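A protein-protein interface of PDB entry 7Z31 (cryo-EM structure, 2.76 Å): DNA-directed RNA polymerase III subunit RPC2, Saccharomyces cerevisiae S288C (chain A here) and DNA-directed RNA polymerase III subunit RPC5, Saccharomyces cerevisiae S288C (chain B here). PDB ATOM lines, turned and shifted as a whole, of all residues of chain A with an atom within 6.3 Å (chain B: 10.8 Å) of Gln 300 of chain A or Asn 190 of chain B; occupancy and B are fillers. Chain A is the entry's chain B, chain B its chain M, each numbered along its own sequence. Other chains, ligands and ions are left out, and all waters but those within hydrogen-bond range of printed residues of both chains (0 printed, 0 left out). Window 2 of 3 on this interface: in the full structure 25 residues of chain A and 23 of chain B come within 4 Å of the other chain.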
ATOM      1  N   ASP A 294      34.922  37.068 -20.238  1.00  0.00           N
ATOM      2  CA  ASP A 294      34.283  36.354 -19.138  1.00  0.00           C
ATOM      3  C   ASP A 294      34.754  34.909 -19.201  1.00  0.00           C
ATOM      4  O   ASP A 294      35.325  34.469 -20.202  1.00  0.00           O
ATOM      5  CB  ASP A 294      32.756  36.430 -19.218  1.00  0.00           C
ATOM      6  CG  ASP A 294      32.225  36.047 -20.582  1.00  0.00           C
ATOM      7  OD1 ASP A 294      32.786  36.510 -21.597  1.00  0.00           O
ATOM      8  OD2 ASP A 294      31.240  35.282 -20.639  1.00  0.00           O
ATOM      9  N   ILE A 295      34.506  34.168 -18.118  1.00  0.00           N
ATOM     10  CA  ILE A 295      34.771  32.737 -18.154  1.00  0.00           C
ATOM     11  C   ILE A 295      33.707  32.067 -19.011  1.00  0.00           C
ATOM     12  O   ILE A 295      32.588  32.576 -19.168  1.00  0.00           O
ATOM     13  CB  ILE A 295      34.828  32.122 -16.746  1.00  0.00           C
ATOM     14  CG1 ILE A 295      35.922  31.058 -16.704  1.00  0.00           C
ATOM     15  CG2 ILE A 295      33.489  31.519 -16.360  1.00  0.00           C
ATOM     16  CD1 ILE A 295      37.269  31.568 -17.152  1.00  0.00           C
ATOM     17  N   TYR A 296      34.061  30.927 -19.595  1.00  0.00           N
ATOM     18  CA  TYR A 296      33.286  30.404 -20.706  1.00  0.00           C
ATOM     19  C   TYR A 296      33.046  28.910 -20.568  1.00  0.00           C
ATOM     20  O   TYR A 296      33.870  28.173 -20.020  1.00  0.00           O
ATOM     21  CB  TYR A 296      33.982  30.690 -22.038  1.00  0.00           C
ATOM     22  CG  TYR A 296      33.411  31.863 -22.794  1.00  0.00           C
ATOM     23  CD1 TYR A 296      32.295  31.712 -23.599  1.00  0.00           C
ATOM     24  CD2 TYR A 296      33.987  33.118 -22.708  1.00  0.00           C
ATOM     25  CE1 TYR A 296      31.765  32.776 -24.294  1.00  0.00           C
ATOM     26  CE2 TYR A 296      33.464  34.186 -23.403  1.00  0.00           C
ATOM     27  CZ  TYR A 296      32.353  34.008 -24.191  1.00  0.00           C
ATOM     28  OH  TYR A 296      31.827  35.066 -24.888  1.00  0.00           O
ATOM     29  N   THR A 297      31.899  28.482 -21.078  1.00  0.00           N
ATOM     30  CA  THR A 297      31.580  27.096 -21.368  1.00  0.00           C
ATOM     31  C   THR A 297      31.501  26.938 -22.881  1.00  0.00           C
ATOM     32  O   THR A 297      31.723  27.887 -23.633  1.00  0.00           O
ATOM     33  CB  THR A 297      30.260  26.683 -20.718  1.00  0.00           C
ATOM     34  OG1 THR A 297      29.182  27.006 -21.606  1.00  0.00           O
ATOM     35  CG2 THR A 297      30.065  27.438 -19.432  1.00  0.00           C
ATOM     36  N   GLN A 298      31.174  25.727 -23.336  1.00  0.00           N
ATOM     37  CA  GLN A 298      31.023  25.517 -24.772  1.00  0.00           C
ATOM     38  C   GLN A 298      29.838  26.299 -25.324  1.00  0.00           C
ATOM     39  O   GLN A 298      29.962  27.000 -26.333  1.00  0.00           O
ATOM     40  CB  GLN A 298      30.871  24.032 -25.088  1.00  0.00           C
ATOM     41  CG  GLN A 298      30.045  23.787 -26.333  1.00  0.00           C
ATOM     42  CD  GLN A 298      30.645  22.755 -27.252  1.00  0.00           C
ATOM     43  OE1 GLN A 298      31.230  21.770 -26.807  1.00  0.00           O
ATOM     44  NE2 GLN A 298      30.496  22.974 -28.553  1.00  0.00           N
ATOM     45  N   GLN A 299      28.674  26.190 -24.677  1.00  0.00           N
ATOM     46  CA  GLN A 299      27.477  26.822 -25.225  1.00  0.00           C
ATOM     47  C   GLN A 299      27.599  28.339 -25.206  1.00  0.00           C
ATOM     48  O   GLN A 299      27.108  29.018 -26.112  1.00  0.00           O
ATOM     49  CB  GLN A 299      26.234  26.367 -24.458  1.00  0.00           C
ATOM     50  CG  GLN A 299      26.180  24.865 -24.143  1.00  0.00           C
ATOM     51  CD  GLN A 299      26.122  23.979 -25.383  1.00  0.00           C
ATOM     52  OE1 GLN A 299      25.571  24.362 -26.415  1.00  0.00           O
ATOM     53  NE2 GLN A 299      26.703  22.787 -25.283  1.00  0.00           N
ATOM     54  N   GLN A 300      28.256  28.893 -24.185  1.00  0.00           N
ATOM     55  CA  GLN A 300      28.490  30.333 -24.151  1.00  0.00           C
ATOM     56  C   GLN A 300      29.342  30.781 -25.334  1.00  0.00           C
ATOM     57  O   GLN A 300      29.049  31.794 -25.983  1.00  0.00           O
ATOM     58  CB  GLN A 300      29.164  30.713 -22.836  1.00  0.00           C
ATOM     59  CG  GLN A 300      28.244  31.287 -21.781  1.00  0.00           C
ATOM     60  CD  GLN A 300      29.025  31.871 -20.624  1.00  0.00           C
ATOM     61  OE1 GLN A 300      28.508  32.668 -19.848  1.00  0.00           O
ATOM     62  NE2 GLN A 300      30.283  31.475 -20.508  1.00  0.00           N
ATOM     63  N   ALA A 301      30.420  30.045 -25.620  1.00  0.00           N
ATOM     64  CA  ALA A 301      31.259  30.387 -26.763  1.00  0.00           C
ATOM     65  C   ALA A 301      30.492  30.245 -28.066  1.00  0.00           C
ATOM     66  O   ALA A 301      30.663  31.055 -28.981  1.00  0.00           O
ATOM     67  CB  ALA A 301      32.510  29.512 -26.774  1.00  0.00           C
ATOM     68  N   LEU A 302      29.635  29.229 -28.158  1.00  0.00           N
ATOM     69  CA  LEU A 302      28.778  29.081 -29.327  1.00  0.00           C
ATOM     70  C   LEU A 302      27.865  30.286 -29.495  1.00  0.00           C
ATOM     71  O   LEU A 302      27.662  30.764 -30.612  1.00  0.00           O
ATOM     72  CB  LEU A 302      27.952  27.802 -29.207  1.00  0.00           C
ATOM     73  CG  LEU A 302      28.718  26.485 -29.266  1.00  0.00           C
ATOM     74  CD1 LEU A 302      27.765  25.292 -29.248  1.00  0.00           C
ATOM     75  CD2 LEU A 302      29.588  26.461 -30.497  1.00  0.00           C
ATOM     76  N   GLU A 303      27.294  30.778 -28.395  1.00  0.00           N
ATOM     77  CA  GLU A 303      26.440  31.960 -28.463  1.00  0.00           C
ATOM     78  C   GLU A 303      27.229  33.180 -28.920  1.00  0.00           C
ATOM     79  O   GLU A 303      26.742  33.983 -29.729  1.00  0.00           O
ATOM     80  CB  GLU A 303      25.794  32.213 -27.101  1.00  0.00           C
ATOM     81  CG  GLU A 303      24.836  31.119 -26.668  1.00  0.00           C
ATOM     82  CD  GLU A 303      24.330  31.303 -25.250  1.00  0.00           C
ATOM     83  OE1 GLU A 303      24.827  32.212 -24.554  1.00  0.00           O
ATOM     84  OE2 GLU A 303      23.433  30.539 -24.833  1.00  0.00           O
ATOM     85  N   TYR A 304      28.453  33.332 -28.416  1.00  0.00           N
ATOM     86  CA  TYR A 304      29.302  34.431 -28.863  1.00  0.00           C
ATOM     87  C   TYR A 304      29.597  34.329 -30.356  1.00  0.00           C
ATOM     88  O   TYR A 304      29.639  35.346 -31.057  1.00  0.00           O
ATOM     89  CB  TYR A 304      30.597  34.460 -28.054  1.00  0.00           C
ATOM     90  CG  TYR A 304      31.468  35.650 -28.368  1.00  0.00           C
ATOM     91  CD1 TYR A 304      30.949  36.932 -28.337  1.00  0.00           C
ATOM     92  CD2 TYR A 304      32.803  35.493 -28.696  1.00  0.00           C
ATOM     93  CE1 TYR A 304      31.735  38.021 -28.619  1.00  0.00           C
ATOM     94  CE2 TYR A 304      33.597  36.578 -28.988  1.00  0.00           C
ATOM     95  CZ  TYR A 304      33.059  37.839 -28.947  1.00  0.00           C
ATOM     96  OH  TYR A 304      33.847  38.926 -29.237  1.00  0.00           O
ATOM     97  N   ILE A 305      29.814  33.111 -30.860  1.00  0.00           N
ATOM     98  CA  ILE A 305      30.000  32.925 -32.299  1.00  0.00           C
ATOM     99  C   ILE A 305      28.728  33.286 -33.054  1.00  0.00           C
ATOM    100  O   ILE A 305      28.770  33.940 -34.102  1.00  0.00           O
ATOM    101  CB  ILE A 305      30.430  31.481 -32.615  1.00  0.00           C
ATOM    102  CG1 ILE A 305      31.708  31.108 -31.872  1.00  0.00           C
ATOM    103  CG2 ILE A 305      30.619  31.300 -34.120  1.00  0.00           C
ATOM    104  CD1 ILE A 305      32.931  31.752 -32.416  1.00  0.00           C
ATOM    105  N   LYS B 135      31.467  32.462  -2.893  1.00  0.00           N
ATOM    106  CA  LYS B 135      31.236  32.745  -4.307  1.00  0.00           C
ATOM    107  C   LYS B 135      30.573  31.567  -5.003  1.00  0.00           C
ATOM    108  O   LYS B 135      29.705  31.770  -5.862  1.00  0.00           O
ATOM    109  CB  LYS B 135      32.548  33.117  -5.000  1.00  0.00           C
ATOM    110  CG  LYS B 135      32.636  32.706  -6.473  1.00  0.00           C
ATOM    111  CD  LYS B 135      33.945  33.163  -7.106  1.00  0.00           C
ATOM    112  CE  LYS B 135      34.144  32.552  -8.490  1.00  0.00           C
ATOM    113  NZ  LYS B 135      33.077  32.959  -9.446  1.00  0.00           N
ATOM    114  N   SER B 138      26.938  31.821  -4.067  1.00  0.00           N
ATOM    115  CA  SER B 138      26.328  33.064  -4.520  1.00  0.00           C
ATOM    116  C   SER B 138      26.112  33.056  -6.028  1.00  0.00           C
ATOM    117  O   SER B 138      25.095  33.562  -6.516  1.00  0.00           O
ATOM    118  CB  SER B 138      27.192  34.253  -4.106  1.00  0.00           C
ATOM    119  OG  SER B 138      28.182  34.527  -5.078  1.00  0.00           O
ATOM    120  N   GLU B 139      27.049  32.479  -6.779  1.00  0.00           N
ATOM    121  CA  GLU B 139      26.943  32.426  -8.230  1.00  0.00           C
ATOM    122  C   GLU B 139      26.072  31.269  -8.708  1.00  0.00           C
ATOM    123  O   GLU B 139      25.126  31.479  -9.472  1.00  0.00           O
ATOM    124  CB  GLU B 139      28.338  32.324  -8.854  1.00  0.00           C
ATOM    125  CG  GLU B 139      28.864  33.628  -9.411  1.00  0.00           C
ATOM    126  CD  GLU B 139      28.953  34.711  -8.363  1.00  0.00           C
ATOM    127  OE1 GLU B 139      29.444  34.419  -7.252  1.00  0.00           O
ATOM    128  OE2 GLU B 139      28.529  35.849  -8.645  1.00  0.00           O
ATOM    129  N   TRP B 140      26.376  30.045  -8.281  1.00  0.00           N
ATOM    130  CA  TRP B 140      25.675  28.867  -8.771  1.00  0.00           C
ATOM    131  C   TRP B 140      25.269  27.993  -7.593  1.00  0.00           C
ATOM    132  O   TRP B 140      26.116  27.600  -6.786  1.00  0.00           O
ATOM    133  CB  TRP B 140      26.555  28.094  -9.757  1.00  0.00           C
ATOM    134  CG  TRP B 140      27.490  28.985 -10.531  1.00  0.00           C
ATOM    135  CD1 TRP B 140      27.150  29.882 -11.501  1.00  0.00           C
ATOM    136  CD2 TRP B 140      28.912  29.070 -10.389  1.00  0.00           C
ATOM    137  NE1 TRP B 140      28.271  30.518 -11.971  1.00  0.00           N
ATOM    138  CE2 TRP B 140      29.366  30.036 -11.306  1.00  0.00           C
ATOM    139  CE3 TRP B 140      29.847  28.418  -9.581  1.00  0.00           C
ATOM    140  CZ2 TRP B 140      30.709  30.367 -11.434  1.00  0.00           C
ATOM    141  CZ3 TRP B 140      31.178  28.749  -9.712  1.00  0.00           C
ATOM    142  CH2 TRP B 140      31.597  29.713 -10.631  1.00  0.00           C
ATOM    143  N   ASN B 141      23.979  27.670  -7.514  1.00  0.00           N
ATOM    144  CA  ASN B 141      23.398  27.045  -6.331  1.00  0.00           C
ATOM    145  C   ASN B 141      24.067  25.722  -5.980  1.00  0.00           C
ATOM    146  O   ASN B 141      24.731  25.613  -4.944  1.00  0.00           O
ATOM    147  CB  ASN B 141      21.904  26.823  -6.547  1.00  0.00           C
ATOM    148  CG  ASN B 141      21.218  28.036  -7.133  1.00  0.00           C
ATOM    149  OD1 ASN B 141      21.574  29.173  -6.830  1.00  0.00           O
ATOM    150  ND2 ASN B 141      20.230  27.799  -7.987  1.00  0.00           N
ATOM    151  N   LYS B 149      31.380  15.812 -19.029  1.00  0.00           N
ATOM    152  CA  LYS B 149      30.511  15.518 -20.159  1.00  0.00           C
ATOM    153  C   LYS B 149      31.353  15.145 -21.369  1.00  0.00           C
ATOM    154  O   LYS B 149      32.395  15.759 -21.619  1.00  0.00           O
ATOM    155  CB  LYS B 149      29.619  16.714 -20.484  1.00  0.00           C
ATOM    156  CG  LYS B 149      28.720  16.509 -21.687  1.00  0.00           C
ATOM    157  CD  LYS B 149      27.983  17.788 -22.025  1.00  0.00           C
ATOM    158  CE  LYS B 149      27.137  17.624 -23.271  1.00  0.00           C
ATOM    159  NZ  LYS B 149      26.546  18.918 -23.707  1.00  0.00           N
ATOM    160  N   PHE B 182      32.517  19.782 -17.314  1.00  0.00           N
ATOM    161  CA  PHE B 182      31.258  20.371 -17.744  1.00  0.00           C
ATOM    162  C   PHE B 182      30.853  21.467 -16.769  1.00  0.00           C
ATOM    163  O   PHE B 182      31.142  21.396 -15.570  1.00  0.00           O
ATOM    164  CB  PHE B 182      30.153  19.311 -17.836  1.00  0.00           C
ATOM    165  CG  PHE B 182      28.950  19.738 -18.628  1.00  0.00           C
ATOM    166  CD1 PHE B 182      29.022  20.781 -19.531  1.00  0.00           C
ATOM    167  CD2 PHE B 182      27.742  19.082 -18.471  1.00  0.00           C
ATOM    168  CE1 PHE B 182      27.913  21.164 -20.260  1.00  0.00           C
ATOM    169  CE2 PHE B 182      26.627  19.460 -19.199  1.00  0.00           C
ATOM    170  CZ  PHE B 182      26.713  20.502 -20.091  1.00  0.00           C
ATOM    171  N   PHE B 183      30.162  22.475 -17.293  1.00  0.00           N
ATOM    172  CA  PHE B 183      29.781  23.650 -16.522  1.00  0.00           C
ATOM    173  C   PHE B 183      28.268  23.810 -16.561  1.00  0.00           C
ATOM    174  O   PHE B 183      27.750  24.876 -16.921  1.00  0.00           O
ATOM    175  CB  PHE B 183      30.469  24.901 -17.059  1.00  0.00           C
ATOM    176  CG  PHE B 183      31.968  24.878 -16.946  1.00  0.00           C
ATOM    177  CD1 PHE B 183      32.600  24.132 -15.968  1.00  0.00           C
ATOM    178  CD2 PHE B 183      32.748  25.616 -17.821  1.00  0.00           C
ATOM    179  CE1 PHE B 183      33.975  24.116 -15.870  1.00  0.00           C
ATOM    180  CE2 PHE B 183      34.127  25.601 -17.721  1.00  0.00           C
ATOM    181  CZ  PHE B 183      34.737  24.850 -16.744  1.00  0.00           C
ATOM    182  N   LYS B 184      27.561  22.724 -16.234  1.00  0.00           N
ATOM    183  CA  LYS B 184      26.101  22.737 -16.218  1.00  0.00           C
ATOM    184  C   LYS B 184      25.558  23.874 -15.366  1.00  0.00           C
ATOM    185  O   LYS B 184      24.570  24.522 -15.734  1.00  0.00           O
ATOM    186  CB  LYS B 184      25.573  21.400 -15.697  1.00  0.00           C
ATOM    187  CG  LYS B 184      24.070  21.369 -15.490  1.00  0.00           C
ATOM    188  CD  LYS B 184      23.330  21.380 -16.818  1.00  0.00           C
ATOM    189  CE  LYS B 184      22.300  20.263 -16.870  1.00  0.00           C
ATOM    190  NZ  LYS B 184      21.759  20.058 -18.241  1.00  0.00           N
ATOM    191  N   TYR B 185      26.171  24.117 -14.206  1.00  0.00           N
ATOM    192  CA  TYR B 185      25.669  25.178 -13.348  1.00  0.00           C
ATOM    193  C   TYR B 185      25.850  26.540 -13.999  1.00  0.00           C
ATOM    194  O   TYR B 185      25.029  27.434 -13.802  1.00  0.00           O
ATOM    195  CB  TYR B 185      26.336  25.137 -11.975  1.00  0.00           C
ATOM    196  CG  TYR B 185      27.834  25.015 -11.987  1.00  0.00           C
ATOM    197  CD1 TYR B 185      28.640  26.121 -12.221  1.00  0.00           C
ATOM    198  CD2 TYR B 185      28.446  23.802 -11.722  1.00  0.00           C
ATOM    199  CE1 TYR B 185      30.012  26.010 -12.220  1.00  0.00           C
ATOM    200  CE2 TYR B 185      29.816  23.685 -11.715  1.00  0.00           C
ATOM    201  CZ  TYR B 185      30.594  24.790 -11.961  1.00  0.00           C
ATOM    202  OH  TYR B 185      31.961  24.668 -11.954  1.00  0.00           O
ATOM    203  N   ILE B 186      26.905  26.715 -14.795  1.00  0.00           N
ATOM    204  CA  ILE B 186      27.049  27.969 -15.526  1.00  0.00           C
ATOM    205  C   ILE B 186      25.985  28.079 -16.607  1.00  0.00           C
ATOM    206  O   ILE B 186      25.407  29.150 -16.817  1.00  0.00           O
ATOM    207  CB  ILE B 186      28.459  28.103 -16.117  1.00  0.00           C
ATOM    208  CG1 ILE B 186      29.504  28.040 -15.015  1.00  0.00           C
ATOM    209  CG2 ILE B 186      28.595  29.420 -16.859  1.00  0.00           C
ATOM    210  CD1 ILE B 186      30.840  28.510 -15.474  1.00  0.00           C
ATOM    211  N   ASP B 187      25.707  26.978 -17.311  1.00  0.00           N
ATOM    212  CA  ASP B 187      24.637  27.005 -18.305  1.00  0.00           C
ATOM    213  C   ASP B 187      23.320  27.441 -17.673  1.00  0.00           C
ATOM    214  O   ASP B 187      22.634  28.329 -18.190  1.00  0.00           O
ATOM    215  CB  ASP B 187      24.489  25.628 -18.959  1.00  0.00           C
ATOM    216  CG  ASP B 187      23.604  25.653 -20.205  1.00  0.00           C
ATOM    217  OD1 ASP B 187      22.408  26.004 -20.092  1.00  0.00           O
ATOM    218  OD2 ASP B 187      24.113  25.326 -21.299  1.00  0.00           O
ATOM    219  N   ASP B 188      22.976  26.860 -16.522  1.00  0.00           N
ATOM    220  CA  ASP B 188      21.680  27.152 -15.913  1.00  0.00           C
ATOM    221  C   ASP B 188      21.669  28.512 -15.214  1.00  0.00           C
ATOM    222  O   ASP B 188      20.646  29.205 -15.217  1.00  0.00           O
ATOM    223  CB  ASP B 188      21.293  26.025 -14.956  1.00  0.00           C
ATOM    224  CG  ASP B 188      20.943  24.741 -15.688  1.00  0.00           C
ATOM    225  OD1 ASP B 188      20.465  24.827 -16.840  1.00  0.00           O
ATOM    226  OD2 ASP B 188      21.138  23.645 -15.119  1.00  0.00           O
ATOM    227  N   ALA B 189      22.792  28.924 -14.621  1.00  0.00           N
ATOM    228  CA  ALA B 189      22.873  30.257 -14.036  1.00  0.00           C
ATOM    229  C   ALA B 189      22.754  31.328 -15.108  1.00  0.00           C
ATOM    230  O   ALA B 189      22.087  32.348 -14.910  1.00  0.00           O
ATOM    231  CB  ALA B 189      24.182  30.417 -13.264  1.00  0.00           C
ATOM    232  N   ASN B 190      23.388  31.110 -16.259  1.00  0.00           N
ATOM    233  CA  ASN B 190      23.235  32.045 -17.363  1.00  0.00           C
ATOM    234  C   ASN B 190      21.819  32.011 -17.915  1.00  0.00           C
ATOM    235  O   ASN B 190      21.295  33.045 -18.339  1.00  0.00           O
ATOM    236  CB  ASN B 190      24.257  31.739 -18.454  1.00  0.00           C
ATOM    237  CG  ASN B 190      25.686  31.992 -18.004  1.00  0.00           C
ATOM    238  OD1 ASN B 190      26.606  31.282 -18.405  1.00  0.00           O
ATOM    239  ND2 ASN B 190      25.876  32.999 -17.159  1.00  0.00           N
ATOM    240  N   VAL B 191      21.179  30.839 -17.913  1.00  0.00           N
ATOM    241  CA  VAL B 191      19.798  30.767 -18.379  1.00  0.00           C
ATOM    242  C   VAL B 191      18.878  31.549 -17.443  1.00  0.00           C
ATOM    243  O   VAL B 191      17.947  32.226 -17.893  1.00  0.00           O
ATOM    244  CB  VAL B 191      19.360  29.296 -18.548  1.00  0.00           C
ATOM    245  CG1 VAL B 191      18.455  28.831 -17.419  1.00  0.00           C
ATOM    246  CG2 VAL B 191      18.672  29.108 -19.890  1.00  0.00           C
ATOM    247  N   THR B 192      19.146  31.505 -16.136  1.00  0.00           N
ATOM    248  CA  THR B 192      18.340  32.279 -15.197  1.00  0.00           C
ATOM    249  C   THR B 192      18.704  33.756 -15.235  1.00  0.00           C
ATOM    250  O   THR B 192      17.891  34.606 -14.859  1.00  0.00           O
ATOM    251  CB  THR B 192      18.487  31.721 -13.780  1.00  0.00           C
ATOM    252  OG1 THR B 192      19.874  31.663 -13.418  1.00  0.00           O
ATOM    253  CG2 THR B 192      17.884  30.321 -13.702  1.00  0.00           C
ATOM    254  N   ARG B 193      19.918  34.081 -15.680  1.00  0.00           N
ATOM    255  CA  ARG B 193      20.254  35.481 -15.907  1.00  0.00           C
ATOM    256  C   ARG B 193      19.533  36.026 -17.135  1.00  0.00           C
ATOM    257  O   ARG B 193      19.069  37.172 -17.132  1.00  0.00           O
ATOM    258  CB  ARG B 193      21.766  35.645 -16.053  1.00  0.00           C
ATOM    259  CG  ARG B 193      22.192  37.082 -16.291  1.00  0.00           C
ATOM    260  CD  ARG B 193      23.611  37.326 -15.824  1.00  0.00           C
ATOM    261  NE  ARG B 193      24.576  36.464 -16.497  1.00  0.00           N
ATOM    262  CZ  ARG B 193      25.154  36.748 -17.657  1.00  0.00           C
ATOM    263  NH1 ARG B 193      24.864  37.855 -18.321  1.00  0.00           N
ATOM    264  NH2 ARG B 193      26.045  35.900 -18.161  1.00  0.00           N
ATOM    265  N   LYS B 194      19.428  35.216 -18.191  1.00  0.00           N
ATOM    266  CA  LYS B 194      18.771  35.646 -19.421  1.00  0.00           C
ATOM    267  C   LYS B 194      17.255  35.498 -19.361  1.00  0.00           C
ATOM    268  O   LYS B 194      16.564  35.994 -20.257  1.00  0.00           O
ATOM    269  CB  LYS B 194      19.295  34.850 -20.622  1.00  0.00           C
ATOM    270  CG  LYS B 194      20.810  34.776 -20.767  1.00  0.00           C
ATOM    271  CD  LYS B 194      21.431  36.101 -21.142  1.00  0.00           C
ATOM    272  CE  LYS B 194      22.950  35.990 -21.162  1.00  0.00           C
ATOM    273  NZ  LYS B 194      23.471  35.302 -19.942  1.00  0.00           N
ATOM    274  N   GLN B 195      16.723  34.817 -18.344  1.00  0.00           N
ATOM    275  CA  GLN B 195      15.280  34.613 -18.271  1.00  0.00           C
ATOM    276  C   GLN B 195      14.500  35.915 -18.131  1.00  0.00           C
ATOM    277  O   GLN B 195      13.283  35.913 -18.348  1.00  0.00           O
ATOM    278  CB  GLN B 195      14.933  33.676 -17.110  1.00  0.00           C
ATOM    279  CG  GLN B 195      14.839  34.355 -15.748  1.00  0.00           C
ATOM    280  CD  GLN B 195      13.798  33.707 -14.854  1.00  0.00           C
ATOM    281  OE1 GLN B 195      13.386  32.573 -15.084  1.00  0.00           O
ATOM    282  NE2 GLN B 195      13.360  34.434 -13.832  1.00  0.00           N
ATOM    283  N   GLU B 196      15.158  37.011 -17.773  1.00  0.00           N
ATOM    284  CA  GLU B 196      14.509  38.312 -17.701  1.00  0.00           C
ATOM    285  C   GLU B 196      15.440  39.391 -18.248  1.00  0.00           C
ATOM    286  O   GLU B 196      16.011  39.242 -19.328  1.00  0.00           O
ATOM    287  CB  GLU B 196      14.104  38.638 -16.261  1.00  0.00           C
ATOM    288  CG  GLU B 196      15.257  39.059 -15.349  1.00  0.00           C
ATOM    289  CD  GLU B 196      16.147  37.905 -14.916  1.00  0.00           C
ATOM    290  OE1 GLU B 196      16.583  37.117 -15.779  1.00  0.00           O
ATOM    291  OE2 GLU B 196      16.415  37.787 -13.703  1.00  0.00           O
ATOM    292  N   HIS B 234      22.005  18.832 -31.826  1.00  0.00           N
ATOM    293  CA  HIS B 234      21.759  19.552 -30.583  1.00  0.00           C
ATOM    294  C   HIS B 234      20.269  19.737 -30.323  1.00  0.00           C
ATOM    295  O   HIS B 234      19.848  19.808 -29.160  1.00  0.00           O
ATOM    296  CB  HIS B 234      22.495  20.889 -30.607  1.00  0.00           C
ATOM    297  CG  HIS B 234      23.964  20.752 -30.858  1.00  0.00           C
ATOM    298  ND1 HIS B 234      24.901  20.828 -29.850  1.00  0.00           N
ATOM    299  CD2 HIS B 234      24.656  20.520 -31.998  1.00  0.00           C
ATOM    300  CE1 HIS B 234      26.108  20.661 -30.360  1.00  0.00           C
ATOM    301  NE2 HIS B 234      25.988  20.472 -31.662  1.00  0.00           N
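Tyr 296 of chain A touches Phe 183 of chain B (O to CE2, 3.5 Å).
Thr 297 of chain A touches Phe 183 of chain B.
Thr 297 of chain A touches Ile 186 of chain B.
Gln 299 of chain A touches Asp 187 of chain B (CG to OD2, 3.5 Å).
Of chain A, only Gln 300 (2.8 Å) comes within 4 Å of Asn 190 of chain B.
Tyr 296 of chain A touches just one residue of chain B: Phe 183 (3.5 Å).
Of the printed residues of chain B, Thr 297 of chain A touches Phe 183 and Ile 186.
Of chain B, only Asp 187 comes within 4 Å of Gln 299 of chain A.
No residue of chain B comes within 4 Å of Ala 301 of chain A.
Leu 302 of chain A touches none of the printed residues of chain B.
No residue of chain B comes within 4 Å of Glu 303 of chain A.
Of the printed residues of chain A, Ile 186 of chain B touches Thr 297.
Of the printed residues of chain A, Phe 183 of chain B touches Tyr 296 (3.5 Å) and Thr 297 (3.5 Å).
Lys 149 of chain B touches none of the printed residues of chain A.
The nearest printed residue of chain B that does not touch Gln 300 of chain A is Arg 193 of chain B (4.4 Å).
Along chain B the printed residues that touch a printed residue of chain A span positions 183 to 190.
Printed residues of chain A that touch a printed residue of chain B: Tyr 296, Thr 297, Gln 299 and Gln 300.
Among the printed residues, 5 pairs touch across the chains.
Among the printed residues, no Asp or Glu carboxylate lies within 4 Å of a Lys or Arg side-chain nitrogen of the other chain.
The side-chain amide nitrogen of Gln 300 of chain A is in hydrogen-bond range of the backbone carbonyl oxygen of Ile 295 of chain A (2.9 Å).
The side-chain hydroxyl of Thr 297 of chain A is in hydrogen-bond range of the backbone NH of Gln 300 of chain A (3.3 Å).
N of Gln 299 of chain A lies within hydrogen-bond range of OG1 of Thr 297 of chain A (3.2 Å).
ND2 of Asn 190 of chain B sits close to NH2 of Arg 193 of chain B (3.1 Å).
The backbone carbonyl oxygen (O) of Ile 186 of chain B sits close to the side-chain amide oxygen (OD1) of Asn 190 of chain B (2.9 Å).
The side-chain amide oxygen (OE1) of Gln 300 of chain A lies close to the side-chain amide oxygen (OD1) of Asn 190 of chain B (2.8 Å).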
